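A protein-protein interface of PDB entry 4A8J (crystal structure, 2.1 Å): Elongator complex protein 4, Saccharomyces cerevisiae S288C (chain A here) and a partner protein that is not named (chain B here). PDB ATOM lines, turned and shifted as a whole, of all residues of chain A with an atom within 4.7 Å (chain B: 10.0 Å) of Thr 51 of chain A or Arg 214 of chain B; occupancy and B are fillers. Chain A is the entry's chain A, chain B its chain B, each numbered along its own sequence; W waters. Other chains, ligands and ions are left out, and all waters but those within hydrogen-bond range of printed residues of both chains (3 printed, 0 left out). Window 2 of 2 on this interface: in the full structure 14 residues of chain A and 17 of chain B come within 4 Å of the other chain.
Hydrophobic or aromatic side chains of chain B that line the printed part of chain A: Leu 216 and Tyr 218.
OE1 of Gln 294 of chain A sits at hydrogen-bond distance from N of Glu 217 of chain B (2.7 Å).
The side-chain hydroxyl (OG1) of Thr 50 of chain A is in hydrogen-bond range of the side-chain hydroxyl (OG) of Ser 215 of chain B, at 2.8 Å.
The side-chain hydroxyl (OG1) of Thr 50 of chain A is in hydrogen-bond range of the backbone carbonyl oxygen (O) of Gly 213 of chain B (2.6 Å).
N of Thr 51 of chain A touches O of Gly 213 of chain B, 3.6 Å away.
Arg 214 of chain B touches Thr 51 of chain A.
Gln 294 of chain A touches Leu 216 of chain B.
Tyr 218 of chain B touches Gln 294 of chain A (CE1 to NE2, 3.7 Å).
Thr 297 of chain A touches Ser 3 of chain B.
Arg 214 of chain B touches Thr 297 of chain A.
Thr 51 of chain A touches two residues of chain B.
Arg 214 of chain B touches just these residues of chain A: Thr 51 and Thr 297.
No residue of chain B comes within 4 Å of Ser 49 of chain A.
No residue of chain B comes within 4 Å of Glu 52 of chain A.
Of the printed residues of chain B, Gln 294 of chain A touches Leu 216, Glu 217 and Tyr 218.
Of the printed residues of chain A, Ser 3 of chain B touches Thr 297 (3.4 Å).
Printed residues of chain A within 4 Å of Tyr 218 of chain B: Gln 294 (3.7 Å).
Of the printed residues of chain A, Ser 215 of chain B touches Thr 50.
Asn 293 of chain A touches none of the printed residues of chain B.
The nearest residue of chain B that does not touch Thr 51 of chain A is Ser 212 of chain B (4.5 Å).
The backbone carbonyl oxygen (O) of Asn 293 of chain A is in hydrogen-bond range of the side-chain hydroxyl (OG1) of Thr 297 of chain A (3.0 Å).
N of Asn 208 of chain B is in hydrogen-bond range of O of Leu 216 of chain B.
OH of Tyr 218 of chain B lies within hydrogen-bond range of N of Ser 5 of chain B (3.0 Å).
The backbone carbonyl oxygen (O) of Ser 3 of chain B is in hydrogen-bond range of the guanidinium group (NH1) of Arg 214 of chain B (2.9 Å).
N of Leu 206 of chain B is in hydrogen-bond range of O of Tyr 218 of chain B, at 2.9 Å.
The side-chain hydroxyl (OG1) of Thr 51 of chain A is in hydrogen-bond range of the side-chain hydroxyl (OG) of Ser 49 of chain A, at 3.3 Å.
Water W1 lies within hydrogen-bond range of the backbone carbonyl oxygen (O) of Ser 212 of chain B (2.7 Å) and the backbone NH (N) of Glu 52 of chain A (2.8 Å).
Water W2 lies within hydrogen-bond range of the guanidinium group (NH2) of Arg 214 of chain B (2.7 Å), the backbone carbonyl oxygen (O) of Asn 293 of chain A (3.4 Å) and the backbone NH (N) of Gln 294 of chain A (3.5 Å).
Water W3 lies within hydrogen-bond range of NH2 of Arg 214 of chain B (2.9 Å), OG of Ser 3 of chain B (3.1 Å) and O of Gln 294 of chain A (3.1 Å).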
ATOM      1  N   GLU A  47     -11.082   2.644 -41.922  1.00  0.00           N
ATOM      2  CA  GLU A  47     -11.614   3.706 -41.068  1.00  0.00           C
ATOM      3  C   GLU A  47     -10.966   3.676 -39.686  1.00  0.00           C
ATOM      4  O   GLU A  47     -10.891   2.624 -39.032  1.00  0.00           O
ATOM      5  CB  GLU A  47     -13.134   3.628 -40.950  1.00  0.00           C
ATOM      6  CG  GLU A  47     -13.774   4.811 -40.195  1.00  0.00           C
ATOM      7  CD  GLU A  47     -15.269   4.963 -40.513  1.00  0.00           C
ATOM      8  OE1 GLU A  47     -15.741   4.288 -41.466  1.00  0.00           O
ATOM      9  OE2 GLU A  47     -15.974   5.753 -39.830  1.00  0.00           O
ATOM     10  N   GLN A  48     -10.467   4.832 -39.262  1.00  0.00           N
ATOM     11  CA  GLN A  48      -9.946   4.996 -37.912  1.00  0.00           C
ATOM     12  C   GLN A  48     -11.114   5.315 -36.963  1.00  0.00           C
ATOM     13  O   GLN A  48     -12.186   5.698 -37.421  1.00  0.00           O
ATOM     14  CB  GLN A  48      -8.908   6.118 -37.890  1.00  0.00           C
ATOM     15  CG  GLN A  48      -7.817   5.939 -38.929  1.00  0.00           C
ATOM     16  CD  GLN A  48      -6.660   6.935 -38.778  1.00  0.00           C
ATOM     17  OE1 GLN A  48      -6.223   7.242 -37.672  1.00  0.00           O
ATOM     18  NE2 GLN A  48      -6.184   7.449 -39.900  1.00  0.00           N
ATOM     19  N   SER A  49     -10.890   5.125 -35.662  1.00  0.00           N
ATOM     20  CA  SER A  49     -11.873   5.362 -34.591  1.00  0.00           C
ATOM     21  C   SER A  49     -13.012   4.347 -34.590  1.00  0.00           C
ATOM     22  O   SER A  49     -12.894   3.279 -35.191  1.00  0.00           O
ATOM     23  CB  SER A  49     -12.420   6.800 -34.602  1.00  0.00           C
ATOM     24  OG  SER A  49     -13.311   7.021 -35.688  1.00  0.00           O
ATOM     25  N   THR A  50     -14.107   4.695 -33.912  1.00  0.00           N
ATOM     26  CA  THR A  50     -15.218   3.779 -33.702  1.00  0.00           C
ATOM     27  C   THR A  50     -16.423   4.080 -34.606  1.00  0.00           C
ATOM     28  O   THR A  50     -17.440   3.388 -34.551  1.00  0.00           O
ATOM     29  CB  THR A  50     -15.657   3.824 -32.234  1.00  0.00           C
ATOM     30  OG1 THR A  50     -15.900   5.187 -31.889  1.00  0.00           O
ATOM     31  CG2 THR A  50     -14.532   3.256 -31.324  1.00  0.00           C
ATOM     32  N   THR A  51     -16.321   5.123 -35.424  1.00  0.00           N
ATOM     33  CA  THR A  51     -17.406   5.459 -36.360  1.00  0.00           C
ATOM     34  C   THR A  51     -17.390   4.512 -37.564  1.00  0.00           C
ATOM     35  O   THR A  51     -16.374   3.854 -37.836  1.00  0.00           O
ATOM     36  CB  THR A  51     -17.300   6.903 -36.855  1.00  0.00           C
ATOM     37  OG1 THR A  51     -16.044   7.074 -37.518  1.00  0.00           O
ATOM     38  CG2 THR A  51     -17.383   7.884 -35.686  1.00  0.00           C
ATOM     39  N   GLU A  52     -18.516   4.428 -38.270  1.00  0.00           N
ATOM     40  CA  GLU A  52     -18.603   3.570 -39.453  1.00  0.00           C
ATOM     41  C   GLU A  52     -19.085   4.320 -40.703  1.00  0.00           C
ATOM     42  O   GLU A  52     -20.059   3.929 -41.355  1.00  0.00           O
ATOM     43  CB  GLU A  52     -19.474   2.332 -39.170  1.00  0.00           C
ATOM     44  CG  GLU A  52     -18.900   1.415 -38.085  1.00  0.00           C
ATOM     45  CD  GLU A  52     -19.619   0.075 -37.972  1.00  0.00           C
ATOM     46  OE1 GLU A  52     -20.752   0.046 -37.433  1.00  0.00           O
ATOM     47  OE2 GLU A  52     -19.043  -0.948 -38.422  1.00  0.00           O
ATOM     48  N   PHE A  53     -18.398   5.405 -41.041  1.00  0.00           N
ATOM     49  CA  PHE A  53     -18.777   6.153 -42.229  1.00  0.00           C
ATOM     50  C   PHE A  53     -18.607   5.252 -43.461  1.00  0.00           C
ATOM     51  O   PHE A  53     -19.308   5.386 -44.471  1.00  0.00           O
ATOM     52  CB  PHE A  53     -17.915   7.404 -42.373  1.00  0.00           C
ATOM     53  CG  PHE A  53     -18.250   8.492 -41.388  1.00  0.00           C
ATOM     54  CD1 PHE A  53     -19.391   9.270 -41.554  1.00  0.00           C
ATOM     55  CD2 PHE A  53     -17.413   8.746 -40.306  1.00  0.00           C
ATOM     56  CE1 PHE A  53     -19.692  10.302 -40.664  1.00  0.00           C
ATOM     57  CE2 PHE A  53     -17.706   9.766 -39.407  1.00  0.00           C
ATOM     58  CZ  PHE A  53     -18.849  10.547 -39.589  1.00  0.00           C
ATOM     59  N   PRO A 291     -11.939  10.148 -39.077  1.00  0.00           N
ATOM     60  CA  PRO A 291     -12.907  11.088 -38.504  1.00  0.00           C
ATOM     61  C   PRO A 291     -12.230  12.132 -37.618  1.00  0.00           C
ATOM     62  O   PRO A 291     -11.247  11.838 -36.926  1.00  0.00           O
ATOM     63  CB  PRO A 291     -13.825  10.179 -37.665  1.00  0.00           C
ATOM     64  CG  PRO A 291     -13.645   8.802 -38.283  1.00  0.00           C
ATOM     65  CD  PRO A 291     -12.194   8.763 -38.644  1.00  0.00           C
ATOM     66  N   ASN A 293     -11.275  14.318 -34.568  1.00  0.00           N
ATOM     67  CA  ASN A 293     -11.343  14.071 -33.121  1.00  0.00           C
ATOM     68  C   ASN A 293     -12.264  15.052 -32.387  1.00  0.00           C
ATOM     69  O   ASN A 293     -12.934  15.872 -33.014  1.00  0.00           O
ATOM     70  CB  ASN A 293      -9.947  14.022 -32.481  1.00  0.00           C
ATOM     71  CG  ASN A 293      -9.194  15.341 -32.575  1.00  0.00           C
ATOM     72  OD1 ASN A 293      -9.778  16.415 -32.749  1.00  0.00           O
ATOM     73  ND2 ASN A 293      -7.877  15.259 -32.454  1.00  0.00           N
ATOM     74  N   GLN A 294     -12.293  14.963 -31.059  1.00  0.00           N
ATOM     75  CA  GLN A 294     -13.246  15.717 -30.239  1.00  0.00           C
ATOM     76  C   GLN A 294     -13.017  17.232 -30.323  1.00  0.00           C
ATOM     77  O   GLN A 294     -13.956  18.011 -30.560  1.00  0.00           O
ATOM     78  CB  GLN A 294     -13.155  15.232 -28.786  1.00  0.00           C
ATOM     79  CG  GLN A 294     -14.294  15.672 -27.882  1.00  0.00           C
ATOM     80  CD  GLN A 294     -14.285  14.957 -26.519  1.00  0.00           C
ATOM     81  OE1 GLN A 294     -13.888  13.793 -26.411  1.00  0.00           O
ATOM     82  NE2 GLN A 294     -14.733  15.656 -25.483  1.00  0.00           N
ATOM     83  N   THR A 297     -13.772  18.602 -33.913  1.00  0.00           N
ATOM     84  CA  THR A 297     -15.219  18.639 -34.109  1.00  0.00           C
ATOM     85  C   THR A 297     -15.817  19.851 -33.378  1.00  0.00           C
ATOM     86  O   THR A 297     -16.601  20.624 -33.955  1.00  0.00           O
ATOM     87  CB  THR A 297     -15.905  17.336 -33.642  1.00  0.00           C
ATOM     88  OG1 THR A 297     -15.488  16.248 -34.485  1.00  0.00           O
ATOM     89  CG2 THR A 297     -17.427  17.479 -33.723  1.00  0.00           C
ATOM     90  N   ALA B   2     -23.506  20.365 -28.966  1.00  0.00           N
ATOM     91  CA  ALA B   2     -24.184  19.139 -29.379  1.00  0.00           C
ATOM     92  C   ALA B   2     -23.195  17.994 -29.624  1.00  0.00           C
ATOM     93  O   ALA B   2     -23.474  16.838 -29.299  1.00  0.00           O
ATOM     94  CB  ALA B   2     -25.039  19.391 -30.629  1.00  0.00           C
ATOM     95  N   SER B   3     -22.043  18.324 -30.199  1.00  0.00           N
ATOM     96  CA  SER B   3     -21.052  17.318 -30.582  1.00  0.00           C
ATOM     97  C   SER B   3     -20.296  16.779 -29.367  1.00  0.00           C
ATOM     98  O   SER B   3     -19.751  15.680 -29.416  1.00  0.00           O
ATOM     99  CB  SER B   3     -20.071  17.882 -31.614  1.00  0.00           C
ATOM    100  OG  SER B   3     -19.071  18.677 -30.997  1.00  0.00           O
ATOM    101  N   SER B   4     -20.264  17.571 -28.295  1.00  0.00           N
ATOM    102  CA  SER B   4     -19.690  17.173 -27.009  1.00  0.00           C
ATOM    103  C   SER B   4     -20.690  17.548 -25.913  1.00  0.00           C
ATOM    104  O   SER B   4     -21.500  18.457 -26.106  1.00  0.00           O
ATOM    105  CB  SER B   4     -18.346  17.866 -26.778  1.00  0.00           C
ATOM    106  OG  SER B   4     -18.069  17.993 -25.393  1.00  0.00           O
ATOM    107  N   SER B   5     -20.645  16.864 -24.769  1.00  0.00           N
ATOM    108  CA  SER B   5     -21.669  17.061 -23.730  1.00  0.00           C
ATOM    109  C   SER B   5     -21.712  18.470 -23.133  1.00  0.00           C
ATOM    110  O   SER B   5     -20.675  19.065 -22.829  1.00  0.00           O
ATOM    111  CB  SER B   5     -21.525  16.040 -22.599  1.00  0.00           C
ATOM    112  OG  SER B   5     -22.594  16.158 -21.670  1.00  0.00           O
ATOM    113  N   LEU B  11     -24.246  13.725 -17.702  1.00  0.00           N
ATOM    114  CA  LEU B  11     -24.014  12.510 -18.487  1.00  0.00           C
ATOM    115  C   LEU B  11     -23.446  11.399 -17.586  1.00  0.00           C
ATOM    116  O   LEU B  11     -23.993  10.290 -17.490  1.00  0.00           O
ATOM    117  CB  LEU B  11     -23.041  12.813 -19.624  1.00  0.00           C
ATOM    118  CG  LEU B  11     -22.650  11.568 -20.428  1.00  0.00           C
ATOM    119  CD1 LEU B  11     -23.913  10.863 -20.971  1.00  0.00           C
ATOM    120  CD2 LEU B  11     -21.691  11.910 -21.550  1.00  0.00           C
ATOM    121  N   PHE B 163     -13.018  -2.250 -27.657  1.00  0.00           N
ATOM    122  CA  PHE B 163     -13.705  -2.151 -28.937  1.00  0.00           C
ATOM    123  C   PHE B 163     -15.191  -2.515 -28.790  1.00  0.00           C
ATOM    124  O   PHE B 163     -16.058  -1.868 -29.366  1.00  0.00           O
ATOM    125  CB  PHE B 163     -13.047  -3.059 -29.997  1.00  0.00           C
ATOM    126  CG  PHE B 163     -13.706  -2.962 -31.352  1.00  0.00           C
ATOM    127  CD1 PHE B 163     -13.331  -1.972 -32.242  1.00  0.00           C
ATOM    128  CD2 PHE B 163     -14.725  -3.834 -31.712  1.00  0.00           C
ATOM    129  CE1 PHE B 163     -13.939  -1.858 -33.497  1.00  0.00           C
ATOM    130  CE2 PHE B 163     -15.345  -3.728 -32.952  1.00  0.00           C
ATOM    131  CZ  PHE B 163     -14.951  -2.736 -33.847  1.00  0.00           C
ATOM    132  N   ALA B 165     -16.990  -2.392 -26.016  1.00  0.00           N
ATOM    133  CA  ALA B 165     -17.688  -1.685 -24.943  1.00  0.00           C
ATOM    134  C   ALA B 165     -18.458  -0.513 -25.506  1.00  0.00           C
ATOM    135  O   ALA B 165     -18.005   0.128 -26.447  1.00  0.00           O
ATOM    136  CB  ALA B 165     -16.719  -1.203 -23.909  1.00  0.00           C
ATOM    137  N   THR B 166     -19.621  -0.237 -24.913  1.00  0.00           N
ATOM    138  CA  THR B 166     -20.396   0.949 -25.270  1.00  0.00           C
ATOM    139  C   THR B 166     -20.006   2.109 -24.363  1.00  0.00           C
ATOM    140  O   THR B 166     -20.139   3.265 -24.733  1.00  0.00           O
ATOM    141  CB  THR B 166     -21.917   0.685 -25.197  1.00  0.00           C
ATOM    142  OG1 THR B 166     -22.243   0.056 -23.954  1.00  0.00           O
ATOM    143  CG2 THR B 166     -22.339  -0.235 -26.333  1.00  0.00           C
ATOM    144  N   THR B 167     -19.510   1.791 -23.172  1.00  0.00           N
ATOM    145  CA  THR B 167     -18.989   2.824 -22.297  1.00  0.00           C
ATOM    146  C   THR B 167     -17.708   2.317 -21.624  1.00  0.00           C
ATOM    147  O   THR B 167     -17.640   1.163 -21.229  1.00  0.00           O
ATOM    148  CB  THR B 167     -20.049   3.208 -21.229  1.00  0.00           C
ATOM    149  OG1 THR B 167     -21.279   3.563 -21.882  1.00  0.00           O
ATOM    150  CG2 THR B 167     -19.567   4.373 -20.381  1.00  0.00           C
ATOM    151  N   LEU B 206     -13.933   8.863 -18.598  1.00  0.00           N
ATOM    152  CA  LEU B 206     -15.117   8.314 -19.230  1.00  0.00           C
ATOM    153  C   LEU B 206     -14.986   8.440 -20.745  1.00  0.00           C
ATOM    154  O   LEU B 206     -14.692   9.510 -21.268  1.00  0.00           O
ATOM    155  CB  LEU B 206     -16.354   9.067 -18.765  1.00  0.00           C
ATOM    156  CG  LEU B 206     -17.677   8.654 -19.418  1.00  0.00           C
ATOM    157  CD1 LEU B 206     -18.138   7.297 -18.902  1.00  0.00           C
ATOM    158  CD2 LEU B 206     -18.762   9.706 -19.162  1.00  0.00           C
ATOM    159  N   VAL B 207     -15.205   7.334 -21.440  1.00  0.00           N
ATOM    160  CA  VAL B 207     -15.375   7.347 -22.887  1.00  0.00           C
ATOM    161  C   VAL B 207     -16.797   6.884 -23.135  1.00  0.00           C
ATOM    162  O   VAL B 207     -17.162   5.747 -22.828  1.00  0.00           O
ATOM    163  CB  VAL B 207     -14.422   6.372 -23.582  1.00  0.00           C
ATOM    164  CG1 VAL B 207     -14.485   6.560 -25.099  1.00  0.00           C
ATOM    165  CG2 VAL B 207     -13.003   6.535 -23.055  1.00  0.00           C
ATOM    166  N   ASN B 208     -17.617   7.787 -23.654  1.00  0.00           N
ATOM    167  CA  ASN B 208     -18.971   7.436 -23.972  1.00  0.00           C
ATOM    168  C   ASN B 208     -19.070   7.269 -25.483  1.00  0.00           C
ATOM    169  O   ASN B 208     -18.731   8.172 -26.263  1.00  0.00           O
ATOM    170  CB  ASN B 208     -19.945   8.481 -23.450  1.00  0.00           C
ATOM    171  CG  ASN B 208     -21.376   8.119 -23.730  1.00  0.00           C
ATOM    172  OD1 ASN B 208     -22.119   8.896 -24.336  1.00  0.00           O
ATOM    173  ND2 ASN B 208     -21.767   6.914 -23.332  1.00  0.00           N
ATOM    174  N   LYS B 209     -19.488   6.086 -25.902  1.00  0.00           N
ATOM    175  CA  LYS B 209     -19.590   5.808 -27.319  1.00  0.00           C
ATOM    176  C   LYS B 209     -21.027   6.052 -27.737  1.00  0.00           C
ATOM    177  O   LYS B 209     -21.904   5.228 -27.449  1.00  0.00           O
ATOM    178  CB  LYS B 209     -19.170   4.368 -27.609  1.00  0.00           C
ATOM    179  CG  LYS B 209     -19.163   4.014 -29.091  1.00  0.00           C
ATOM    180  CD  LYS B 209     -18.306   2.777 -29.333  1.00  0.00           C
ATOM    181  CE  LYS B 209     -19.099   1.649 -29.993  1.00  0.00           C
ATOM    182  NZ  LYS B 209     -18.919   0.346 -29.268  1.00  0.00           N
ATOM    183  N   ARG B 210     -21.264   7.192 -28.399  1.00  0.00           N
ATOM    184  CA  ARG B 210     -22.618   7.585 -28.843  1.00  0.00           C
ATOM    185  C   ARG B 210     -23.210   6.652 -29.910  1.00  0.00           C
ATOM    186  O   ARG B 210     -22.484   5.851 -30.526  1.00  0.00           O
ATOM    187  CB  ARG B 210     -22.597   9.013 -29.390  1.00  0.00           C
ATOM    188  CG  ARG B 210     -22.165  10.071 -28.396  1.00  0.00           C
ATOM    189  CD  ARG B 210     -22.150  11.438 -29.068  1.00  0.00           C
ATOM    190  NE  ARG B 210     -22.070  12.544 -28.117  1.00  0.00           N
ATOM    191  CZ  ARG B 210     -22.259  13.822 -28.436  1.00  0.00           C
ATOM    192  NH1 ARG B 210     -22.531  14.163 -29.695  1.00  0.00           N
ATOM    193  NH2 ARG B 210     -22.178  14.759 -27.494  1.00  0.00           N
ATOM    194  N   LYS B 211     -24.519   6.777 -30.146  1.00  0.00           N
ATOM    195  CA  LYS B 211     -25.205   6.005 -31.196  1.00  0.00           C
ATOM    196  C   LYS B 211     -24.609   6.297 -32.552  1.00  0.00           C
ATOM    197  O   LYS B 211     -24.648   5.453 -33.431  1.00  0.00           O
ATOM    198  CB  LYS B 211     -26.691   6.383 -31.322  1.00  0.00           C
ATOM    199  N   SER B 212     -24.118   7.519 -32.732  1.00  0.00           N
ATOM    200  CA  SER B 212     -23.562   7.953 -34.011  1.00  0.00           C
ATOM    201  C   SER B 212     -22.262   7.203 -34.289  1.00  0.00           C
ATOM    202  O   SER B 212     -21.775   7.162 -35.427  1.00  0.00           O
ATOM    203  CB  SER B 212     -23.291   9.457 -33.976  1.00  0.00           C
ATOM    204  OG  SER B 212     -22.246   9.739 -33.054  1.00  0.00           O
ATOM    205  N   GLY B 213     -21.698   6.615 -33.238  1.00  0.00           N
ATOM    206  CA  GLY B 213     -20.434   5.898 -33.363  1.00  0.00           C
ATOM    207  C   GLY B 213     -19.267   6.705 -32.824  1.00  0.00           C
ATOM    208  O   GLY B 213     -18.209   6.143 -32.542  1.00  0.00           O
ATOM    209  N   ARG B 214     -19.451   8.020 -32.673  1.00  0.00           N
ATOM    210  CA  ARG B 214     -18.381   8.863 -32.113  1.00  0.00           C
ATOM    211  C   ARG B 214     -18.131   8.559 -30.623  1.00  0.00           C
ATOM    212  O   ARG B 214     -19.063   8.352 -29.845  1.00  0.00           O
ATOM    213  CB  ARG B 214     -18.687  10.357 -32.302  1.00  0.00           C
ATOM    214  CG  ARG B 214     -18.635  10.802 -33.745  1.00  0.00           C
ATOM    215  CD  ARG B 214     -18.764  12.304 -33.893  1.00  0.00           C
ATOM    216  NE  ARG B 214     -17.756  13.055 -33.146  1.00  0.00           N
ATOM    217  CZ  ARG B 214     -18.049  13.919 -32.179  1.00  0.00           C
ATOM    218  NH1 ARG B 214     -19.316  14.123 -31.852  1.00  0.00           N
ATOM    219  NH2 ARG B 214     -17.083  14.585 -31.555  1.00  0.00           N
ATOM    220  N   SER B 215     -16.858   8.516 -30.257  1.00  0.00           N
ATOM    221  CA  SER B 215     -16.430   8.242 -28.902  1.00  0.00           C
ATOM    222  C   SER B 215     -15.960   9.542 -28.280  1.00  0.00           C
ATOM    223  O   SER B 215     -14.998  10.153 -28.756  1.00  0.00           O
ATOM    224  CB  SER B 215     -15.290   7.213 -28.899  1.00  0.00           C
ATOM    225  OG  SER B 215     -15.808   5.916 -29.141  1.00  0.00           O
ATOM    226  N   LEU B 216     -16.644   9.963 -27.221  1.00  0.00           N
ATOM    227  CA  LEU B 216     -16.280  11.199 -26.527  1.00  0.00           C
ATOM    228  C   LEU B 216     -15.649  10.939 -25.161  1.00  0.00           C
ATOM    229  O   LEU B 216     -16.085  10.067 -24.433  1.00  0.00           O
ATOM    230  CB  LEU B 216     -17.497  12.112 -26.416  1.00  0.00           C
ATOM    231  CG  LEU B 216     -17.704  12.758 -27.796  1.00  0.00           C
ATOM    232  CD1 LEU B 216     -19.025  12.374 -28.395  1.00  0.00           C
ATOM    233  CD2 LEU B 216     -17.511  14.269 -27.739  1.00  0.00           C
ATOM    234  N   GLU B 217     -14.634  11.722 -24.819  1.00  0.00           N
ATOM    235  CA  GLU B 217     -13.851  11.494 -23.612  1.00  0.00           C
ATOM    236  C   GLU B 217     -13.984  12.662 -22.632  1.00  0.00           C
ATOM    237  O   GLU B 217     -13.955  13.816 -23.040  1.00  0.00           O
ATOM    238  CB  GLU B 217     -12.385  11.345 -24.006  1.00  0.00           C
ATOM    239  CG  GLU B 217     -11.660  10.159 -23.408  1.00  0.00           C
ATOM    240  CD  GLU B 217     -10.262  10.010 -23.993  1.00  0.00           C
ATOM    241  OE1 GLU B 217      -9.444  10.945 -23.829  1.00  0.00           O
ATOM    242  OE2 GLU B 217      -9.994   8.972 -24.640  1.00  0.00           O
ATOM    243  N   TYR B 218     -14.102  12.354 -21.344  1.00  0.00           N
ATOM    244  CA  TYR B 218     -14.126  13.372 -20.291  1.00  0.00           C
ATOM    245  C   TYR B 218     -13.441  12.864 -19.015  1.00  0.00           C
ATOM    246  O   TYR B 218     -13.605  11.706 -18.647  1.00  0.00           O
ATOM    247  CB  TYR B 218     -15.563  13.734 -19.943  1.00  0.00           C
ATOM    248  CG  TYR B 218     -16.496  13.903 -21.124  1.00  0.00           C
ATOM    249  CD1 TYR B 218     -16.507  15.071 -21.857  1.00  0.00           C
ATOM    250  CD2 TYR B 218     -17.382  12.894 -21.486  1.00  0.00           C
ATOM    251  CE1 TYR B 218     -17.375  15.235 -22.929  1.00  0.00           C
ATOM    252  CE2 TYR B 218     -18.250  13.043 -22.554  1.00  0.00           C
ATOM    253  CZ  TYR B 218     -18.245  14.212 -23.272  1.00  0.00           C
ATOM    254  OH  TYR B 218     -19.114  14.359 -24.344  1.00  0.00           O
HETATM  255  O   HOH W   1     -20.775   5.043 -36.692  1.00  0.00           O
HETATM  256  O   HOH W   2     -14.948  13.240 -32.522  1.00  0.00           O
HETATM  257  O   HOH W   3     -16.814  16.938 -29.809  1.00  0.00           O
